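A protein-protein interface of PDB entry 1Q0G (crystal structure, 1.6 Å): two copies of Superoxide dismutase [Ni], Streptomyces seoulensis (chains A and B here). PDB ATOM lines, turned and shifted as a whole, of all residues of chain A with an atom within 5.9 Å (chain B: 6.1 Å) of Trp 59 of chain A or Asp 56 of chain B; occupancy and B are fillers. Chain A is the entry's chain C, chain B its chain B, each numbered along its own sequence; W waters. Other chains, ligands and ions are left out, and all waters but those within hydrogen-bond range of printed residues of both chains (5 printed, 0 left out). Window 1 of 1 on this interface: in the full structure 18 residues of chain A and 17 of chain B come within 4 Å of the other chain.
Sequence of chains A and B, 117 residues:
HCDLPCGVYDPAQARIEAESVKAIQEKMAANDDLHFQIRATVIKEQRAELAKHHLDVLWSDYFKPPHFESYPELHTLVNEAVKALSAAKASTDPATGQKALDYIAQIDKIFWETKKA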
ATOM      1  N   HIS A  53      36.737  -9.224 -24.436  1.00  0.00           N
ATOM      2  CA  HIS A  53      37.208  -8.186 -25.340  1.00  0.00           C
ATOM      3  C   HIS A  53      37.241  -8.681 -26.784  1.00  0.00           C
ATOM      4  O   HIS A  53      36.787  -7.993 -27.695  1.00  0.00           O
ATOM      5  CB  HIS A  53      38.611  -7.728 -24.942  1.00  0.00           C
ATOM      6  CG  HIS A  53      39.232  -6.786 -25.924  1.00  0.00           C
ATOM      7  ND1 HIS A  53      38.744  -5.515 -26.147  1.00  0.00           N
ATOM      8  CD2 HIS A  53      40.276  -6.941 -26.771  1.00  0.00           C
ATOM      9  CE1 HIS A  53      39.461  -4.930 -27.088  1.00  0.00           C
ATOM     10  NE2 HIS A  53      40.397  -5.773 -27.484  1.00  0.00           N
ATOM     11  N   HIS A  54      37.780  -9.878 -26.989  1.00  0.00           N
ATOM     12  CA  HIS A  54      37.868 -10.423 -28.337  1.00  0.00           C
ATOM     13  C   HIS A  54      36.494 -10.616 -28.958  1.00  0.00           C
ATOM     14  O   HIS A  54      36.308 -10.356 -30.145  1.00  0.00           O
ATOM     15  CB  HIS A  54      38.644 -11.742 -28.333  1.00  0.00           C
ATOM     16  CG  HIS A  54      40.103 -11.572 -28.046  1.00  0.00           C
ATOM     17  ND1 HIS A  54      40.887 -10.652 -28.708  1.00  0.00           N
ATOM     18  CD2 HIS A  54      40.924 -12.210 -27.176  1.00  0.00           C
ATOM     19  CE1 HIS A  54      42.128 -10.730 -28.259  1.00  0.00           C
ATOM     20  NE2 HIS A  54      42.177 -11.667 -27.329  1.00  0.00           N
ATOM     21  N   LEU A  55      35.534 -11.068 -28.162  1.00  0.00           N
ATOM     22  CA  LEU A  55      34.187 -11.262 -28.682  1.00  0.00           C
ATOM     23  C   LEU A  55      33.560  -9.903 -28.979  1.00  0.00           C
ATOM     24  O   LEU A  55      32.871  -9.739 -29.990  1.00  0.00           O
ATOM     25  CB  LEU A  55      33.326 -12.051 -27.690  1.00  0.00           C
ATOM     26  CG  LEU A  55      33.711 -13.525 -27.493  1.00  0.00           C
ATOM     27  CD1 LEU A  55      32.787 -14.165 -26.471  1.00  0.00           C
ATOM     28  CD2 LEU A  55      33.622 -14.268 -28.823  1.00  0.00           C
ATOM     29  N   ASP A  56      33.807  -8.926 -28.108  1.00  0.00           N
ATOM     30  CA  ASP A  56      33.272  -7.584 -28.317  1.00  0.00           C
ATOM     31  C   ASP A  56      33.780  -7.020 -29.642  1.00  0.00           C
ATOM     32  O   ASP A  56      33.043  -6.342 -30.357  1.00  0.00           O
ATOM     33  CB  ASP A  56      33.680  -6.638 -27.183  1.00  0.00           C
ATOM     34  CG  ASP A  56      32.924  -6.899 -25.893  1.00  0.00           C
ATOM     35  OD1 ASP A  56      31.885  -7.593 -25.928  1.00  0.00           O
ATOM     36  OD2 ASP A  56      33.369  -6.393 -24.838  1.00  0.00           O
ATOM     37  N   VAL A  57      35.044  -7.292 -29.958  1.00  0.00           N
ATOM     38  CA  VAL A  57      35.644  -6.819 -31.201  1.00  0.00           C
ATOM     39  C   VAL A  57      34.982  -7.464 -32.417  1.00  0.00           C
ATOM     40  O   VAL A  57      34.736  -6.792 -33.414  1.00  0.00           O
ATOM     41  CB  VAL A  57      37.174  -7.095 -31.225  1.00  0.00           C
ATOM     42  CG1 VAL A  57      37.734  -6.878 -32.626  1.00  0.00           C
ATOM     43  CG2 VAL A  57      37.875  -6.162 -30.248  1.00  0.00           C
ATOM     44  N   LEU A  58      34.694  -8.762 -32.341  1.00  0.00           N
ATOM     45  CA  LEU A  58      34.037  -9.440 -33.459  1.00  0.00           C
ATOM     46  C   LEU A  58      32.659  -8.819 -33.642  1.00  0.00           C
ATOM     47  O   LEU A  58      32.235  -8.531 -34.763  1.00  0.00           O
ATOM     48  CB  LEU A  58      33.876 -10.934 -33.177  1.00  0.00           C
ATOM     49  CG  LEU A  58      35.141 -11.792 -33.179  1.00  0.00           C
ATOM     50  CD1 LEU A  58      34.799 -13.213 -32.756  1.00  0.00           C
ATOM     51  CD2 LEU A  58      35.759 -11.776 -34.566  1.00  0.00           C
ATOM     52  N   TRP A  59      31.978  -8.606 -32.520  1.00  0.00           N
ATOM     53  CA  TRP A  59      30.635  -8.032 -32.513  1.00  0.00           C
ATOM     54  C   TRP A  59      30.566  -6.606 -33.058  1.00  0.00           C
ATOM     55  O   TRP A  59      29.703  -6.290 -33.876  1.00  0.00           O
ATOM     56  CB  TRP A  59      30.078  -8.052 -31.083  1.00  0.00           C
ATOM     57  CG  TRP A  59      28.683  -7.488 -30.945  1.00  0.00           C
ATOM     58  CD1 TRP A  59      27.512  -8.089 -31.314  1.00  0.00           C
ATOM     59  CD2 TRP A  59      28.325  -6.215 -30.393  1.00  0.00           C
ATOM     60  NE1 TRP A  59      26.444  -7.269 -31.022  1.00  0.00           N
ATOM     61  CE2 TRP A  59      26.915  -6.112 -30.458  1.00  0.00           C
ATOM     62  CE3 TRP A  59      29.058  -5.151 -29.848  1.00  0.00           C
ATOM     63  CZ2 TRP A  59      26.224  -4.984 -30.000  1.00  0.00           C
ATOM     64  CZ3 TRP A  59      28.371  -4.032 -29.392  1.00  0.00           C
ATOM     65  CH2 TRP A  59      26.964  -3.959 -29.471  1.00  0.00           C
ATOM     66  N   SER A  60      31.469  -5.742 -32.606  1.00  0.00           N
ATOM     67  CA  SER A  60      31.455  -4.346 -33.035  1.00  0.00           C
ATOM     68  C   SER A  60      32.169  -4.046 -34.346  1.00  0.00           C
ATOM     69  O   SER A  60      31.730  -3.190 -35.115  1.00  0.00           O
ATOM     70  CB  SER A  60      32.069  -3.460 -31.950  1.00  0.00           C
ATOM     71  OG  SER A  60      33.454  -3.735 -31.796  1.00  0.00           O
ATOM     72  N   ASP A  61      33.268  -4.747 -34.598  1.00  0.00           N
ATOM     73  CA  ASP A  61      34.062  -4.497 -35.793  1.00  0.00           C
ATOM     74  C   ASP A  61      33.875  -5.463 -36.963  1.00  0.00           C
ATOM     75  O   ASP A  61      33.635  -5.027 -38.089  1.00  0.00           O
ATOM     76  CB  ASP A  61      35.545  -4.458 -35.416  1.00  0.00           C
ATOM     77  CG  ASP A  61      35.878  -3.344 -34.431  1.00  0.00           C
ATOM     78  OD1 ASP A  61      34.951  -2.720 -33.871  1.00  0.00           O
ATOM     79  OD2 ASP A  61      37.081  -3.097 -34.213  1.00  0.00           O
ATOM     80  N   TYR A  62      33.998  -6.762 -36.717  1.00  0.00           N
ATOM     81  CA  TYR A  62      33.867  -7.719 -37.811  1.00  0.00           C
ATOM     82  C   TYR A  62      32.462  -7.830 -38.381  1.00  0.00           C
ATOM     83  O   TYR A  62      32.238  -7.562 -39.564  1.00  0.00           O
ATOM     84  CB  TYR A  62      34.365  -9.112 -37.398  1.00  0.00           C
ATOM     85  CG  TYR A  62      34.088 -10.087 -38.511  1.00  0.00           C
ATOM     86  CD1 TYR A  62      34.884 -10.096 -39.658  1.00  0.00           C
ATOM     87  CD2 TYR A  62      33.026 -11.013 -38.465  1.00  0.00           C
ATOM     88  CE1 TYR A  62      34.611 -10.936 -40.738  1.00  0.00           C
ATOM     89  CE2 TYR A  62      32.746 -11.857 -39.539  1.00  0.00           C
ATOM     90  CZ  TYR A  62      33.540 -11.810 -40.671  1.00  0.00           C
ATOM     91  OH  TYR A  62      33.268 -12.646 -41.722  1.00  0.00           O
ATOM     92  N   PHE A  63      31.516  -8.239 -37.544  1.00  0.00           N
ATOM     93  CA  PHE A  63      30.147  -8.402 -38.002  1.00  0.00           C
ATOM     94  C   PHE A  63      29.541  -7.079 -38.430  1.00  0.00           C
ATOM     95  O   PHE A  63      29.586  -6.090 -37.701  1.00  0.00           O
ATOM     96  CB  PHE A  63      29.299  -9.065 -36.917  1.00  0.00           C
ATOM     97  CG  PHE A  63      29.630 -10.518 -36.694  1.00  0.00           C
ATOM     98  CD1 PHE A  63      29.503 -11.446 -37.730  1.00  0.00           C
ATOM     99  CD2 PHE A  63      30.063 -10.962 -35.448  1.00  0.00           C
ATOM    100  CE1 PHE A  63      29.804 -12.794 -37.523  1.00  0.00           C
ATOM    101  CE2 PHE A  63      30.365 -12.306 -35.233  1.00  0.00           C
ATOM    102  CZ  PHE A  63      30.235 -13.222 -36.273  1.00  0.00           C
ATOM    103  N   LYS A  64      28.984  -7.071 -39.636  1.00  0.00           N
ATOM    104  CA  LYS A  64      28.370  -5.877 -40.199  1.00  0.00           C
ATOM    105  C   LYS A  64      26.849  -5.957 -40.059  1.00  0.00           C
ATOM    106  O   LYS A  64      26.301  -7.024 -39.806  1.00  0.00           O
ATOM    107  CB  LYS A  64      28.767  -5.746 -41.671  1.00  0.00           C
ATOM    108  CG  LYS A  64      30.277  -5.713 -41.912  1.00  0.00           C
ATOM    109  CD  LYS A  64      30.941  -4.566 -41.157  1.00  0.00           C
ATOM    110  CE  LYS A  64      32.420  -4.428 -41.511  1.00  0.00           C
ATOM    111  NZ  LYS A  64      33.206  -5.648 -41.175  1.00  0.00           N
ATOM    112  N   PHE A  68      23.740  -9.376 -38.917  1.00  0.00           N
ATOM    113  CA  PHE A  68      22.781  -9.495 -37.833  1.00  0.00           C
ATOM    114  C   PHE A  68      21.375  -9.740 -38.369  1.00  0.00           C
ATOM    115  O   PHE A  68      20.502 -10.211 -37.647  1.00  0.00           O
ATOM    116  CB  PHE A  68      22.832  -8.238 -36.963  1.00  0.00           C
ATOM    117  CG  PHE A  68      24.142  -8.066 -36.235  1.00  0.00           C
ATOM    118  CD1 PHE A  68      24.497  -8.940 -35.210  1.00  0.00           C
ATOM    119  CD2 PHE A  68      25.023  -7.047 -36.585  1.00  0.00           C
ATOM    120  CE1 PHE A  68      25.717  -8.800 -34.541  1.00  0.00           C
ATOM    121  CE2 PHE A  68      26.249  -6.897 -35.922  1.00  0.00           C
ATOM    122  CZ  PHE A  68      26.592  -7.777 -34.897  1.00  0.00           C
ATOM    123  N   LEU A  74      22.247 -13.774 -33.778  1.00  0.00           N
ATOM    124  CA  LEU A  74      23.615 -13.333 -33.514  1.00  0.00           C
ATOM    125  C   LEU A  74      23.819 -12.363 -32.348  1.00  0.00           C
ATOM    126  O   LEU A  74      24.682 -12.601 -31.504  1.00  0.00           O
ATOM    127  CB  LEU A  74      24.239 -12.757 -34.789  1.00  0.00           C
ATOM    128  CG  LEU A  74      25.755 -12.528 -34.744  1.00  0.00           C
ATOM    129  CD1 LEU A  74      26.467 -13.806 -34.300  1.00  0.00           C
ATOM    130  CD2 LEU A  74      26.241 -12.096 -36.117  1.00  0.00           C
ATOM    131  N   HIS A  75      23.056 -11.274 -32.291  1.00  0.00           N
ATOM    132  CA  HIS A  75      23.216 -10.331 -31.179  1.00  0.00           C
ATOM    133  C   HIS A  75      23.060 -11.045 -29.840  1.00  0.00           C
ATOM    134  O   HIS A  75      23.894 -10.902 -28.943  1.00  0.00           O
ATOM    135  CB  HIS A  75      22.183  -9.202 -31.250  1.00  0.00           C
ATOM    136  CG  HIS A  75      22.537  -8.102 -32.201  1.00  0.00           C
ATOM    137  ND1 HIS A  75      23.703  -7.371 -32.097  1.00  0.00           N
ATOM    138  CD2 HIS A  75      21.856  -7.576 -33.247  1.00  0.00           C
ATOM    139  CE1 HIS A  75      23.721  -6.441 -33.035  1.00  0.00           C
ATOM    140  NE2 HIS A  75      22.612  -6.545 -33.746  1.00  0.00           N
ATOM    141  N   VAL A  78      26.090 -13.519 -29.058  1.00  0.00           N
ATOM    142  CA  VAL A  78      27.310 -12.897 -28.556  1.00  0.00           C
ATOM    143  C   VAL A  78      27.082 -12.352 -27.147  1.00  0.00           C
ATOM    144  O   VAL A  78      27.951 -12.476 -26.282  1.00  0.00           O
ATOM    145  CB  VAL A  78      27.795 -11.751 -29.470  1.00  0.00           C
ATOM    146  CG1 VAL A  78      29.080 -11.146 -28.902  1.00  0.00           C
ATOM    147  CG2 VAL A  78      28.039 -12.273 -30.884  1.00  0.00           C
ATOM    148  N   ALA B  51      35.996   4.876 -25.440  1.00  0.00           N
ATOM    149  CA  ALA B  51      34.554   5.083 -25.558  1.00  0.00           C
ATOM    150  C   ALA B  51      33.864   3.791 -25.997  1.00  0.00           C
ATOM    151  O   ALA B  51      32.812   3.427 -25.469  1.00  0.00           O
ATOM    152  CB  ALA B  51      34.257   6.209 -26.550  1.00  0.00           C
ATOM    153  N   LYS B  52      34.463   3.097 -26.963  1.00  0.00           N
ATOM    154  CA  LYS B  52      33.899   1.842 -27.446  1.00  0.00           C
ATOM    155  C   LYS B  52      33.856   0.823 -26.309  1.00  0.00           C
ATOM    156  O   LYS B  52      32.868   0.113 -26.137  1.00  0.00           O
ATOM    157  CB  LYS B  52      34.726   1.292 -28.616  1.00  0.00           C
ATOM    158  CG  LYS B  52      34.609   2.100 -29.900  1.00  0.00           C
ATOM    159  CD  LYS B  52      35.471   1.498 -31.012  1.00  0.00           C
ATOM    160  CE  LYS B  52      35.004   0.097 -31.391  1.00  0.00           C
ATOM    161  NZ  LYS B  52      35.949  -0.566 -32.338  1.00  0.00           N
ATOM    162  N   HIS B  53      34.925   0.766 -25.521  1.00  0.00           N
ATOM    163  CA  HIS B  53      34.980  -0.166 -24.407  1.00  0.00           C
ATOM    164  C   HIS B  53      33.845   0.080 -23.414  1.00  0.00           C
ATOM    165  O   HIS B  53      33.172  -0.856 -22.991  1.00  0.00           O
ATOM    166  CB  HIS B  53      36.320  -0.048 -23.678  1.00  0.00           C
ATOM    167  CG  HIS B  53      36.393  -0.868 -22.429  1.00  0.00           C
ATOM    168  ND1 HIS B  53      36.288  -2.241 -22.436  1.00  0.00           N
ATOM    169  CD2 HIS B  53      36.528  -0.506 -21.132  1.00  0.00           C
ATOM    170  CE1 HIS B  53      36.356  -2.691 -21.194  1.00  0.00           C
ATOM    171  NE2 HIS B  53      36.501  -1.659 -20.384  1.00  0.00           N
ATOM    172  N   HIS B  54      33.640   1.342 -23.041  1.00  0.00           N
ATOM    173  CA  HIS B  54      32.585   1.678 -22.094  1.00  0.00           C
ATOM    174  C   HIS B  54      31.212   1.271 -22.615  1.00  0.00           C
ATOM    175  O   HIS B  54      30.386   0.765 -21.854  1.00  0.00           O
ATOM    176  CB  HIS B  54      32.603   3.177 -21.779  1.00  0.00           C
ATOM    177  CG  HIS B  54      33.817   3.617 -21.022  1.00  0.00           C
ATOM    178  ND1 HIS B  54      34.247   2.982 -19.875  1.00  0.00           N
ATOM    179  CD2 HIS B  54      34.673   4.645 -21.227  1.00  0.00           C
ATOM    180  CE1 HIS B  54      35.315   3.603 -19.407  1.00  0.00           C
ATOM    181  NE2 HIS B  54      35.594   4.616 -20.208  1.00  0.00           N
ATOM    182  N   LEU B  55      30.961   1.490 -23.903  1.00  0.00           N
ATOM    183  CA  LEU B  55      29.670   1.103 -24.462  1.00  0.00           C
ATOM    184  C   LEU B  55      29.543  -0.413 -24.470  1.00  0.00           C
ATOM    185  O   LEU B  55      28.476  -0.952 -24.175  1.00  0.00           O
ATOM    186  CB  LEU B  55      29.493   1.657 -25.880  1.00  0.00           C
ATOM    187  CG  LEU B  55      29.352   3.181 -25.977  1.00  0.00           C
ATOM    188  CD1 LEU B  55      29.111   3.584 -27.427  1.00  0.00           C
ATOM    189  CD2 LEU B  55      28.196   3.648 -25.092  1.00  0.00           C
ATOM    190  N   ASP B  56      30.634  -1.102 -24.800  1.00  0.00           N
ATOM    191  CA  ASP B  56      30.622  -2.563 -24.823  1.00  0.00           C
ATOM    192  C   ASP B  56      30.252  -3.101 -23.444  1.00  0.00           C
ATOM    193  O   ASP B  56      29.518  -4.080 -23.325  1.00  0.00           O
ATOM    194  CB  ASP B  56      31.995  -3.125 -25.221  1.00  0.00           C
ATOM    195  CG  ASP B  56      32.314  -2.934 -26.694  1.00  0.00           C
ATOM    196  OD1 ASP B  56      31.390  -2.646 -27.486  1.00  0.00           O
ATOM    197  OD2 ASP B  56      33.498  -3.093 -27.065  1.00  0.00           O
ATOM    198  N   VAL B  57      30.778  -2.463 -22.404  1.00  0.00           N
ATOM    199  CA  VAL B  57      30.503  -2.877 -21.032  1.00  0.00           C
ATOM    200  C   VAL B  57      29.029  -2.694 -20.674  1.00  0.00           C
ATOM    201  O   VAL B  57      28.438  -3.546 -20.013  1.00  0.00           O
ATOM    202  CB  VAL B  57      31.387  -2.094 -20.026  1.00  0.00           C
ATOM    203  CG1 VAL B  57      30.899  -2.321 -18.599  1.00  0.00           C
ATOM    204  CG2 VAL B  57      32.837  -2.549 -20.151  1.00  0.00           C
ATOM    205  N   LEU B  58      28.427  -1.590 -21.107  1.00  0.00           N
ATOM    206  CA  LEU B  58      27.013  -1.371 -20.808  1.00  0.00           C
ATOM    207  C   LEU B  58      26.196  -2.479 -21.463  1.00  0.00           C
ATOM    208  O   LEU B  58      25.297  -3.054 -20.854  1.00  0.00           O
ATOM    209  CB  LEU B  58      26.542  -0.013 -21.345  1.00  0.00           C
ATOM    210  CG  LEU B  58      27.040   1.257 -20.651  1.00  0.00           C
ATOM    211  CD1 LEU B  58      26.508   2.478 -21.385  1.00  0.00           C
ATOM    212  CD2 LEU B  58      26.583   1.268 -19.200  1.00  0.00           C
ATOM    213  N   TRP B  59      26.538  -2.776 -22.711  1.00  0.00           N
ATOM    214  CA  TRP B  59      25.854  -3.794 -23.495  1.00  0.00           C
ATOM    215  C   TRP B  59      26.029  -5.214 -22.950  1.00  0.00           C
ATOM    216  O   TRP B  59      25.067  -5.977 -22.857  1.00  0.00           O
ATOM    217  CB  TRP B  59      26.361  -3.732 -24.941  1.00  0.00           C
ATOM    218  CG  TRP B  59      25.782  -4.776 -25.845  1.00  0.00           C
ATOM    219  CD1 TRP B  59      24.538  -4.776 -26.413  1.00  0.00           C
ATOM    220  CD2 TRP B  59      26.420  -5.984 -26.273  1.00  0.00           C
ATOM    221  NE1 TRP B  59      24.364  -5.913 -27.171  1.00  0.00           N
ATOM    222  CE2 TRP B  59      25.503  -6.672 -27.101  1.00  0.00           C
ATOM    223  CE3 TRP B  59      27.679  -6.554 -26.036  1.00  0.00           C
ATOM    224  CZ2 TRP B  59      25.806  -7.901 -27.693  1.00  0.00           C
ATOM    225  CZ3 TRP B  59      27.979  -7.781 -26.628  1.00  0.00           C
ATOM    226  CH2 TRP B  59      27.044  -8.439 -27.445  1.00  0.00           C
ATOM    227  N   SER B  60      27.256  -5.567 -22.581  1.00  0.00           N
ATOM    228  CA  SER B  60      27.530  -6.913 -22.092  1.00  0.00           C
ATOM    229  C   SER B  60      27.229  -7.148 -20.621  1.00  0.00           C
ATOM    230  O   SER B  60      26.792  -8.230 -20.244  1.00  0.00           O
ATOM    231  CB  SER B  60      28.997  -7.269 -22.339  1.00  0.00           C
ATOM    232  OG  SER B  60      29.848  -6.473 -21.531  1.00  0.00           O
ATOM    233  N   ASP B  61      27.461  -6.133 -19.795  1.00  0.00           N
ATOM    234  CA  ASP B  61      27.273  -6.275 -18.359  1.00  0.00           C
ATOM    235  C   ASP B  61      26.004  -5.673 -17.755  1.00  0.00           C
ATOM    236  O   ASP B  61      25.276  -6.358 -17.037  1.00  0.00           O
ATOM    237  CB  ASP B  61      28.490  -5.696 -17.631  1.00  0.00           C
ATOM    238  CG  ASP B  61      29.788  -6.431 -17.957  1.00  0.00           C
ATOM    239  OD1 ASP B  61      29.831  -7.251 -18.902  1.00  0.00           O
ATOM    240  OD2 ASP B  61      30.785  -6.174 -17.255  1.00  0.00           O
ATOM    241  N   HIS B  75      20.058  -3.611 -29.178  1.00  0.00           N
ATOM    242  CA  HIS B  75      21.244  -4.276 -29.725  1.00  0.00           C
ATOM    243  C   HIS B  75      21.828  -3.491 -30.893  1.00  0.00           C
ATOM    244  O   HIS B  75      23.022  -3.185 -30.918  1.00  0.00           O
ATOM    245  CB  HIS B  75      20.913  -5.692 -30.210  1.00  0.00           C
ATOM    246  CG  HIS B  75      20.833  -6.710 -29.117  1.00  0.00           C
ATOM    247  ND1 HIS B  75      21.879  -6.965 -28.257  1.00  0.00           N
ATOM    248  CD2 HIS B  75      19.843  -7.566 -28.769  1.00  0.00           C
ATOM    249  CE1 HIS B  75      21.537  -7.933 -27.426  1.00  0.00           C
ATOM    250  NE2 HIS B  75      20.306  -8.316 -27.716  1.00  0.00           N
ATOM    251  N   THR B  76      20.982  -3.173 -31.868  1.00  0.00           N
ATOM    252  CA  THR B  76      21.426  -2.430 -33.041  1.00  0.00           C
ATOM    253  C   THR B  76      21.915  -1.031 -32.675  1.00  0.00           C
ATOM    254  O   THR B  76      22.881  -0.535 -33.252  1.00  0.00           O
ATOM    255  CB  THR B  76      20.292  -2.321 -34.084  1.00  0.00           C
ATOM    256  OG1 THR B  76      19.957  -3.631 -34.556  1.00  0.00           O
ATOM    257  CG2 THR B  76      20.724  -1.463 -35.258  1.00  0.00           C
ATOM    258  N   VAL B  78      23.371   0.078 -29.808  1.00  0.00           N
ATOM    259  CA  VAL B  78      24.717   0.065 -29.248  1.00  0.00           C
ATOM    260  C   VAL B  78      25.722  -0.315 -30.333  1.00  0.00           C
ATOM    261  O   VAL B  78      26.800   0.265 -30.415  1.00  0.00           O
ATOM    262  CB  VAL B  78      24.841  -0.925 -28.068  1.00  0.00           C
ATOM    263  CG1 VAL B  78      26.249  -0.848 -27.472  1.00  0.00           C
ATOM    264  CG2 VAL B  78      23.809  -0.592 -27.000  1.00  0.00           C
ATOM    265  N   ASN B  79      25.359  -1.281 -31.174  1.00  0.00           N
ATOM    266  CA  ASN B  79      26.256  -1.716 -32.237  1.00  0.00           C
ATOM    267  C   ASN B  79      26.569  -0.575 -33.200  1.00  0.00           C
ATOM    268  O   ASN B  79      27.713  -0.412 -33.627  1.00  0.00           O
ATOM    269  CB  ASN B  79      25.646  -2.897 -32.996  1.00  0.00           C
ATOM    270  CG  ASN B  79      26.671  -3.646 -33.825  1.00  0.00           C
ATOM    271  OD1 ASN B  79      26.759  -3.473 -35.041  1.00  0.00           O
ATOM    272  ND2 ASN B  79      27.465  -4.485 -33.160  1.00  0.00           N
ATOM    273  N   GLU B  80      25.557   0.219 -33.547  1.00  0.00           N
ATOM    274  CA  GLU B  80      25.769   1.343 -34.452  1.00  0.00           C
ATOM    275  C   GLU B  80      26.588   2.430 -33.756  1.00  0.00           C
ATOM    276  O   GLU B  80      27.358   3.143 -34.395  1.00  0.00           O
ATOM    277  CB  GLU B  80      24.429   1.928 -34.920  1.00  0.00           C
ATOM    278  CG  GLU B  80      23.547   0.947 -35.684  1.00  0.00           C
ATOM    279  CD  GLU B  80      22.280   1.595 -36.231  1.00  0.00           C
ATOM    280  OE1 GLU B  80      21.663   2.406 -35.506  1.00  0.00           O
ATOM    281  OE2 GLU B  80      21.898   1.283 -37.381  1.00  0.00           O
ATOM    282  N   VAL B  82      29.009   1.975 -31.470  1.00  0.00           N
ATOM    283  CA  VAL B  82      30.421   1.616 -31.469  1.00  0.00           C
ATOM    284  C   VAL B  82      30.996   1.706 -32.877  1.00  0.00           C
ATOM    285  O   VAL B  82      32.149   2.082 -33.056  1.00  0.00           O
ATOM    286  CB  VAL B  82      30.656   0.210 -30.865  1.00  0.00           C
ATOM    287  CG1 VAL B  82      30.265   0.219 -29.388  1.00  0.00           C
ATOM    288  CG2 VAL B  82      29.858  -0.838 -31.616  1.00  0.00           C
ATOM    289  N   LYS B  83      30.188   1.374 -33.880  1.00  0.00           N
ATOM    290  CA  LYS B  83      30.641   1.470 -35.260  1.00  0.00           C
ATOM    291  C   LYS B  83      30.855   2.942 -35.616  1.00  0.00           C
ATOM    292  O   LYS B  83      31.730   3.279 -36.415  1.00  0.00           O
ATOM    293  CB  LYS B  83      29.617   0.825 -36.204  1.00  0.00           C
ATOM    294  CG  LYS B  83      29.726  -0.698 -36.271  1.00  0.00           C
ATOM    295  CD  LYS B  83      28.613  -1.321 -37.103  1.00  0.00           C
ATOM    296  CE  LYS B  83      28.923  -2.773 -37.459  1.00  0.00           C
ATOM    297  NZ  LYS B  83      29.228  -3.628 -36.271  1.00  0.00           N
HETATM  298  O   HOH W   1      32.474  -6.751 -22.385  1.00  0.00           O
HETATM  299  O   HOH W   2      36.170  -5.631 -22.941  1.00  0.00           O
HETATM  300  O   HOH W   3      35.599  -4.184 -25.090  1.00  0.00           O
HETATM  301  O   HOH W   4      22.092  -4.804 -35.944  1.00  0.00           O
HETATM  302  O   HOH W   5      34.498  -2.846 -29.440  1.00  0.00           O
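Hydrophobic or aromatic side chains of chain B within 4 Å of the printed part of chain A: Trp 59, His 75, Val 78 and Val 82. Along chain B the printed residues that touch a printed residue of chain A span positions 52 to 83. Of the 16 printed residues of chain A, 8 touch a printed residue of chain B. Printed residues of chain A that touch a printed residue of chain B: Asp 56, Trp 59, Ser 60, Asp 61, Phe 63, Phe 68, His 75 and Val 78. Hydrophobic or aromatic side chains of chain A within 4 Å of the printed part of chain B: Trp 59, Phe 68, His 75 and Val 78.
Among the printed residues, pairs that only touch across the chains: Asp 56 of chain A with Asp 56 of chain B (3.6 Å), Asp 56 of chain A with Trp 59 of chain B (3.97 Å), Trp 59 of chain A with Asp 56 of chain B (3.8 Å), Trp 59 of chain A with Trp 59 of chain B (3.4 Å), Trp 59 of chain A with His 75 of chain B (3.8 Å), Trp 59 of chain A with Val 78 of chain B (3.8 Å), Trp 59 of chain A with Lys 83 of chain B (3.6 Å), Ser 60 of chain A with Asn 79 of chain B (3.99 Å), Ser 60 of chain A with Val 82 of chain B (3.4 Å), Phe 68 of chain A with Asn 79 of chain B (3.6 Å), His 75 of chain A with Trp 59 of chain B (3.8 Å), His 75 of chain A with His 75 of chain B (3.5 Å) and Val 78 of chain A with Trp 59 of chain B (3.7 Å).
NZ of Lys 52 of chain B is in salt-bridge range of OD1 of Asp 61 of chain A (2.8 Å). The side-chain amide nitrogen (ND2) of Asn 79 of chain B lies within hydrogen-bond range of the backbone carbonyl oxygen (O) of Trp 59 of chain A. The side-chain amino group (NZ) of Lys 83 of chain B sits at hydrogen-bond distance from the backbone carbonyl oxygen (O) of Ser 60 of chain A (2.8 Å). The side-chain amino group (NZ) of Lys 83 of chain B is in hydrogen-bond range of the backbone carbonyl oxygen (O) of Phe 63 of chain A, at 2.9 Å.
O of Asp 56 of chain A sits at hydrogen-bond distance from OG of Ser 60 of chain A, at 3.0 Å. OD1 of Asp 61 of chain A is in hydrogen-bond range of OG of Ser 60 of chain A (2.8 Å). The side-chain amino group of Lys 64 of chain A sits at hydrogen-bond distance from the backbone carbonyl oxygen of Asp 61 of chain A, at 3.2 Å.
Water W4 bridges the side-chain hydroxyl (OG1) of Thr 76 of chain B (2.8 Å) and a ring nitrogen (NE2) of His 75 of chain A (2.9 Å). Water W2 lies within hydrogen-bond range of a ring nitrogen (ND1) of His 53 of chain B and the side-chain carboxylate (OD2) of Asp 56 of chain A.
Trp 59 of chain A touches its own counterpart, Trp 59 of chain B. Trp 59 of chain A touches His 75 of chain B, and with the chains exchanged His 75 of chain A touches Trp 59 of chain B. Trp 59 of chain A touches Val 78 of chain B, and with the chains exchanged Val 78 of chain A touches Trp 59 of chain B. 11 positions are printed for both chains.
Trp 59 of chain A touches just these residues of chain B: Asp 56, Trp 59, His 75, Val 78, Asn 79 and Lys 83. Printed residues of chain B within 4 Å of Val 78 of chain A: Trp 59 (3.7 Å). Of chain A, only Asp 56 and Trp 59 come within 4 Å of Asp 56 of chain B. Of the printed residues of chain A, Trp 59 of chain B touches Asp 56, Trp 59, His 75 and Val 78. Printed residues of chain A within 4 Å of Lys 83 of chain B: Trp 59, Ser 60 and Phe 63.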
